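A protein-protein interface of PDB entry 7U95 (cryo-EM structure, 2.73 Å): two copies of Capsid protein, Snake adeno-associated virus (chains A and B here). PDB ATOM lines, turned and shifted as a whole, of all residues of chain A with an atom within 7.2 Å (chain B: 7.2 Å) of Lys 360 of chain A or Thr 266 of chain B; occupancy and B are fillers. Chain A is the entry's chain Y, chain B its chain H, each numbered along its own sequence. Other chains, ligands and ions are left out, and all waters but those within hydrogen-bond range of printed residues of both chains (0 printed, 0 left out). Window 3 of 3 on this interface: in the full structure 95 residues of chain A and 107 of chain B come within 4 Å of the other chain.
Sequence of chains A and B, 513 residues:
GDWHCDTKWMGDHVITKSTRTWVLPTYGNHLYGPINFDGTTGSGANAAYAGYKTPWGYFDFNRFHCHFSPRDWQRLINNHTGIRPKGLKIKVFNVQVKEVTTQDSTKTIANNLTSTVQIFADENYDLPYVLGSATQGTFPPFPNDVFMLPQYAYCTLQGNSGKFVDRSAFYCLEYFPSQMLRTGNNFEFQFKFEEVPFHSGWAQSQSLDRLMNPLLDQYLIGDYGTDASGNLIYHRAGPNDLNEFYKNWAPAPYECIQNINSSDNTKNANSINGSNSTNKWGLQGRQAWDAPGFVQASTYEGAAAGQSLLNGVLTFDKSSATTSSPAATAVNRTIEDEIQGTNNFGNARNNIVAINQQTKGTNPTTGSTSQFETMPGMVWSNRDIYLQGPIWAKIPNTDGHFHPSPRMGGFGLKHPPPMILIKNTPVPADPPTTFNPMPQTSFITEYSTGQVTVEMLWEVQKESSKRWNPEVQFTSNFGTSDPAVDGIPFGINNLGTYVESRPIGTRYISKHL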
ATOM      1  N   ALA A 228       8.597  15.307   1.527  1.00  0.00           N
ATOM      2  CA  ALA A 228       7.328  15.290   0.818  1.00  0.00           C
ATOM      3  C   ALA A 228       7.513  15.003  -0.660  1.00  0.00           C
ATOM      4  O   ALA A 228       6.554  14.613  -1.330  1.00  0.00           O
ATOM      5  CB  ALA A 228       6.599  16.617   1.000  1.00  0.00           C
ATOM      6  N   SER A 229       8.717  15.203  -1.183  1.00  0.00           N
ATOM      7  CA  SER A 229       9.035  14.899  -2.567  1.00  0.00           C
ATOM      8  C   SER A 229       9.692  13.542  -2.736  1.00  0.00           C
ATOM      9  O   SER A 229       9.913  13.121  -3.871  1.00  0.00           O
ATOM     10  CB  SER A 229       9.946  15.979  -3.143  1.00  0.00           C
ATOM     11  OG  SER A 229       9.295  17.235  -3.150  1.00  0.00           O
ATOM     12  N   GLY A 230       9.989  12.840  -1.646  1.00  0.00           N
ATOM     13  CA  GLY A 230      10.635  11.546  -1.712  1.00  0.00           C
ATOM     14  C   GLY A 230      12.090  11.523  -1.310  1.00  0.00           C
ATOM     15  O   GLY A 230      12.717  10.466  -1.411  1.00  0.00           O
ATOM     16  N   ASN A 231      12.652  12.637  -0.860  1.00  0.00           N
ATOM     17  CA  ASN A 231      14.062  12.705  -0.507  1.00  0.00           C
ATOM     18  C   ASN A 231      14.297  12.221   0.915  1.00  0.00           C
ATOM     19  O   ASN A 231      13.515  12.513   1.820  1.00  0.00           O
ATOM     20  CB  ASN A 231      14.579  14.133  -0.650  1.00  0.00           C
ATOM     21  CG  ASN A 231      14.543  14.619  -2.067  1.00  0.00           C
ATOM     22  OD1 ASN A 231      14.029  15.695  -2.352  1.00  0.00           O
ATOM     23  ND2 ASN A 231      15.098  13.832  -2.971  1.00  0.00           N
ATOM     24  N   GLN A 358       8.712  -1.029  -0.364  1.00  0.00           N
ATOM     25  CA  GLN A 358       8.149   0.254  -0.748  1.00  0.00           C
ATOM     26  C   GLN A 358       8.532   0.634  -2.176  1.00  0.00           C
ATOM     27  O   GLN A 358       9.467   0.093  -2.769  1.00  0.00           O
ATOM     28  CB  GLN A 358       8.623   1.377   0.156  1.00  0.00           C
ATOM     29  CG  GLN A 358      10.040   1.734  -0.134  1.00  0.00           C
ATOM     30  CD  GLN A 358      10.453   3.020   0.482  1.00  0.00           C
ATOM     31  OE1 GLN A 358       9.827   3.498   1.414  1.00  0.00           O
ATOM     32  NE2 GLN A 358      11.502   3.613  -0.051  1.00  0.00           N
ATOM     33  N   THR A 359       7.787   1.585  -2.712  1.00  0.00           N
ATOM     34  CA  THR A 359       8.067   2.272  -3.969  1.00  0.00           C
ATOM     35  C   THR A 359       7.162   3.497  -3.977  1.00  0.00           C
ATOM     36  O   THR A 359       6.536   3.810  -2.960  1.00  0.00           O
ATOM     37  CB  THR A 359       7.872   1.348  -5.172  1.00  0.00           C
ATOM     38  OG1 THR A 359       8.322   2.007  -6.362  1.00  0.00           O
ATOM     39  CG2 THR A 359       6.414   0.953  -5.327  1.00  0.00           C
ATOM     40  N   LYS A 360       7.100   4.215  -5.102  1.00  0.00           N
ATOM     41  CA  LYS A 360       6.278   5.424  -5.156  1.00  0.00           C
ATOM     42  C   LYS A 360       4.847   5.166  -4.712  1.00  0.00           C
ATOM     43  O   LYS A 360       4.296   5.909  -3.894  1.00  0.00           O
ATOM     44  CB  LYS A 360       6.273   6.019  -6.559  1.00  0.00           C
ATOM     45  CG  LYS A 360       7.580   6.590  -6.989  1.00  0.00           C
ATOM     46  CD  LYS A 360       8.042   7.610  -5.983  1.00  0.00           C
ATOM     47  CE  LYS A 360       7.214   8.864  -6.005  1.00  0.00           C
ATOM     48  NZ  LYS A 360       7.794   9.858  -5.071  1.00  0.00           N
ATOM     49  N   GLY A 361       4.223   4.132  -5.246  1.00  0.00           N
ATOM     50  CA  GLY A 361       2.829   3.905  -4.938  1.00  0.00           C
ATOM     51  C   GLY A 361       2.594   3.319  -3.565  1.00  0.00           C
ATOM     52  O   GLY A 361       1.617   3.664  -2.898  1.00  0.00           O
ATOM     53  N   THR A 362       3.487   2.440  -3.125  1.00  0.00           N
ATOM     54  CA  THR A 362       3.261   1.621  -1.943  1.00  0.00           C
ATOM     55  C   THR A 362       3.953   2.240  -0.739  1.00  0.00           C
ATOM     56  O   THR A 362       5.166   2.465  -0.764  1.00  0.00           O
ATOM     57  CB  THR A 362       3.768   0.201  -2.166  1.00  0.00           C
ATOM     58  OG1 THR A 362       5.171   0.240  -2.428  1.00  0.00           O
ATOM     59  CG2 THR A 362       3.068  -0.424  -3.349  1.00  0.00           C
ATOM     60  N   ASN A 363       3.190   2.501   0.306  1.00  0.00           N
ATOM     61  CA  ASN A 363       3.764   2.956   1.554  1.00  0.00           C
ATOM     62  C   ASN A 363       4.330   1.769   2.323  1.00  0.00           C
ATOM     63  O   ASN A 363       3.789   0.665   2.252  1.00  0.00           O
ATOM     64  CB  ASN A 363       2.710   3.653   2.396  1.00  0.00           C
ATOM     65  CG  ASN A 363       2.132   4.859   1.713  1.00  0.00           C
ATOM     66  OD1 ASN A 363       0.919   5.026   1.654  1.00  0.00           O
ATOM     67  ND2 ASN A 363       2.996   5.709   1.186  1.00  0.00           N
ATOM     68  N   ASN B 261      15.934   4.485  -0.811  1.00  0.00           N
ATOM     69  CA  ASN B 261      16.879   4.847  -1.852  1.00  0.00           C
ATOM     70  C   ASN B 261      17.460   6.210  -1.519  1.00  0.00           C
ATOM     71  O   ASN B 261      16.726   7.197  -1.427  1.00  0.00           O
ATOM     72  CB  ASN B 261      16.204   4.852  -3.220  1.00  0.00           C
ATOM     73  CG  ASN B 261      17.184   4.989  -4.349  1.00  0.00           C
ATOM     74  OD1 ASN B 261      18.252   5.562  -4.193  1.00  0.00           O
ATOM     75  ND2 ASN B 261      16.849   4.416  -5.486  1.00  0.00           N
ATOM     76  N   SER B 263      20.043   7.925  -3.299  1.00  0.00           N
ATOM     77  CA  SER B 263      20.269   8.772  -4.464  1.00  0.00           C
ATOM     78  C   SER B 263      18.973   9.164  -5.163  1.00  0.00           C
ATOM     79  O   SER B 263      18.677  10.352  -5.320  1.00  0.00           O
ATOM     80  CB  SER B 263      21.205   8.066  -5.445  1.00  0.00           C
ATOM     81  OG  SER B 263      22.492   7.889  -4.883  1.00  0.00           O
ATOM     82  N   ASP B 264      18.177   8.181  -5.577  1.00  0.00           N
ATOM     83  CA  ASP B 264      17.081   8.422  -6.511  1.00  0.00           C
ATOM     84  C   ASP B 264      15.839   8.868  -5.757  1.00  0.00           C
ATOM     85  O   ASP B 264      15.315   8.137  -4.915  1.00  0.00           O
ATOM     86  CB  ASP B 264      16.772   7.181  -7.343  1.00  0.00           C
ATOM     87  CG  ASP B 264      17.851   6.877  -8.357  1.00  0.00           C
ATOM     88  OD1 ASP B 264      18.682   7.770  -8.627  1.00  0.00           O
ATOM     89  OD2 ASP B 264      17.873   5.746  -8.886  1.00  0.00           O
ATOM     90  N   ASN B 265      15.364  10.063  -6.088  1.00  0.00           N
ATOM     91  CA  ASN B 265      14.187  10.616  -5.436  1.00  0.00           C
ATOM     92  C   ASN B 265      12.945   9.796  -5.758  1.00  0.00           C
ATOM     93  O   ASN B 265      12.080   9.600  -4.901  1.00  0.00           O
ATOM     94  CB  ASN B 265      14.017  12.062  -5.892  1.00  0.00           C
ATOM     95  CG  ASN B 265      13.001  12.806  -5.095  1.00  0.00           C
ATOM     96  OD1 ASN B 265      12.191  12.214  -4.398  1.00  0.00           O
ATOM     97  ND2 ASN B 265      13.024  14.123  -5.199  1.00  0.00           N
ATOM     98  N   THR B 266      12.851   9.292  -6.981  1.00  0.00           N
ATOM     99  CA  THR B 266      11.617   8.727  -7.502  1.00  0.00           C
ATOM    100  C   THR B 266      11.403   7.277  -7.106  1.00  0.00           C
ATOM    101  O   THR B 266      10.444   6.664  -7.575  1.00  0.00           O
ATOM    102  CB  THR B 266      11.603   8.835  -9.023  1.00  0.00           C
ATOM    103  OG1 THR B 266      12.712   8.109  -9.558  1.00  0.00           O
ATOM    104  CG2 THR B 266      11.731  10.279  -9.437  1.00  0.00           C
ATOM    105  N   LYS B 267      12.289   6.702  -6.307  1.00  0.00           N
ATOM    106  CA  LYS B 267      12.137   5.333  -5.847  1.00  0.00           C
ATOM    107  C   LYS B 267      11.536   5.235  -4.453  1.00  0.00           C
ATOM    108  O   LYS B 267      11.327   4.123  -3.966  1.00  0.00           O
ATOM    109  CB  LYS B 267      13.489   4.625  -5.867  1.00  0.00           C
ATOM    110  CG  LYS B 267      14.163   4.618  -7.217  1.00  0.00           C
ATOM    111  CD  LYS B 267      13.353   3.874  -8.235  1.00  0.00           C
ATOM    112  CE  LYS B 267      14.083   3.808  -9.554  1.00  0.00           C
ATOM    113  NZ  LYS B 267      13.276   3.110 -10.585  1.00  0.00           N
ATOM    114  N   ASN B 268      11.261   6.358  -3.799  1.00  0.00           N
ATOM    115  CA  ASN B 268      10.816   6.378  -2.415  1.00  0.00           C
ATOM    116  C   ASN B 268       9.397   6.903  -2.321  1.00  0.00           C
ATOM    117  O   ASN B 268       9.040   7.871  -2.994  1.00  0.00           O
ATOM    118  CB  ASN B 268      11.717   7.257  -1.554  1.00  0.00           C
ATOM    119  CG  ASN B 268      13.118   6.744  -1.466  1.00  0.00           C
ATOM    120  OD1 ASN B 268      14.070   7.492  -1.626  1.00  0.00           O
ATOM    121  ND2 ASN B 268      13.259   5.458  -1.212  1.00  0.00           N
ATOM    122  N   ALA B 269       8.600   6.284  -1.463  1.00  0.00           N
ATOM    123  CA  ALA B 269       7.264   6.786  -1.205  1.00  0.00           C
ATOM    124  C   ALA B 269       7.339   8.155  -0.547  1.00  0.00           C
ATOM    125  O   ALA B 269       8.316   8.497   0.118  1.00  0.00           O
ATOM    126  CB  ALA B 269       6.493   5.820  -0.314  1.00  0.00           C
ATOM    127  N   ASN B 270       6.293   8.945  -0.745  1.00  0.00           N
ATOM    128  CA  ASN B 270       6.270  10.299  -0.217  1.00  0.00           C
ATOM    129  C   ASN B 270       5.931  10.285   1.265  1.00  0.00           C
ATOM    130  O   ASN B 270       4.952   9.663   1.681  1.00  0.00           O
ATOM    131  CB  ASN B 270       5.257  11.146  -0.975  1.00  0.00           C
ATOM    132  CG  ASN B 270       5.680  11.424  -2.391  1.00  0.00           C
ATOM    133  OD1 ASN B 270       6.860  11.386  -2.716  1.00  0.00           O
ATOM    134  ND2 ASN B 270       4.714  11.702  -3.250  1.00  0.00           N
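The side-chain amide nitrogen (ND2) of Asn 268 of chain B sits close to the side-chain amide nitrogen (NE2) of Gln 358 of chain A (2.8 Å). The side-chain amide oxygen (OD1) of Asn 268 of chain B lies close to the backbone carbonyl oxygen (O) of Gly 230 of chain A (3.3 Å). The side-chain amide oxygen (OD1) of Asn 265 of chain B sits close to the backbone carbonyl oxygen (O) of Ser 229 of chain A (2.5 Å). The side-chain amino group of Lys 360 of chain A is in hydrogen-bond range of the backbone carbonyl oxygen of Asn 268 of chain B (3.1 Å). The side-chain amide nitrogen (ND2) of Asn 265 of chain B sits close to the side-chain amide nitrogen (ND2) of Asn 231 of chain A, 3.1 Å away. The side-chain amide oxygen (OD1) of Asn 270 of chain B sits at hydrogen-bond distance from the side-chain amino group (NZ) of Lys 360 of chain A (3.0 Å).
The backbone carbonyl oxygen of Asn 261 of chain B lies close to the side-chain amide oxygen of Asn 268 of chain B (2.7 Å). The side-chain hydroxyl of Thr 362 of chain A lies within hydrogen-bond range of the backbone NH of Thr 359 of chain A (3.0 Å).
Ala 228 of chain A touches Asn 270 of chain B. OD1 of Asn 270 of chain B touches C of Ser 229 of chain A (3.6 Å). C of Gly 230 of chain A touches OD1 of Asn 265 of chain B, at 3.2 Å. N of Gly 230 of chain A touches OD1 of Asn 270 of chain B (3.6 Å). O of Lys 267 of chain B touches NE2 of Gln 358 of chain A, 3.95 Å away. Thr 359 of chain A touches Lys 267 of chain B (CA to O, 3.7 Å). O of Thr 359 of chain A touches CB of Ala 269 of chain B, at 3.3 Å. Thr 266 of chain B touches Lys 360 of chain A. O of Thr 362 of chain A touches CB of Ala 269 of chain B, 3.6 Å away. Asn 363 of chain A touches Ala 269 of chain B.
Of chain B, only Thr 266, Asn 268 and Asn 270 come within 4 Å of Lys 360 of chain A. Thr 266 of chain B touches just one residue of chain A: Lys 360. Printed residues of chain A within 4 Å of Asn 265 of chain B: Ser 229 (2.5 Å), Gly 230 (3.2 Å) and Asn 231 (3.1 Å). Printed residues of chain A within 4 Å of Asn 270 of chain B: Ala 228, Ser 229, Gly 230 and Lys 360. Printed residues of chain A within 4 Å of Ala 269 of chain B: Thr 359 (3.3 Å), Thr 362 (3.6 Å) and Asn 363 (3.8 Å). Gly 361 of chain A touches none of the printed residues of chain B. Asn 261 of chain B touches none of the printed residues of chain A. The nearest residue of chain B that does not touch Lys 360 of chain A is Ala 269 of chain B (4.1 Å). The nearest residue of chain A that does not touch Thr 266 of chain B is Thr 359 of chain A (5.3 Å).
Of the 9 printed residues of chain B, 6 touch a printed residue of chain A. Among the printed residues, 16 pairs touch across the chains. Among the printed residues, no Asp or Glu carboxylate lies within 4 Å of a Lys or Arg side-chain nitrogen of the other chain.
No position is printed for both chains. Of the 16 pairs that touch across the chains among the printed residues, none has its exchanged pair printed and touching as well.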
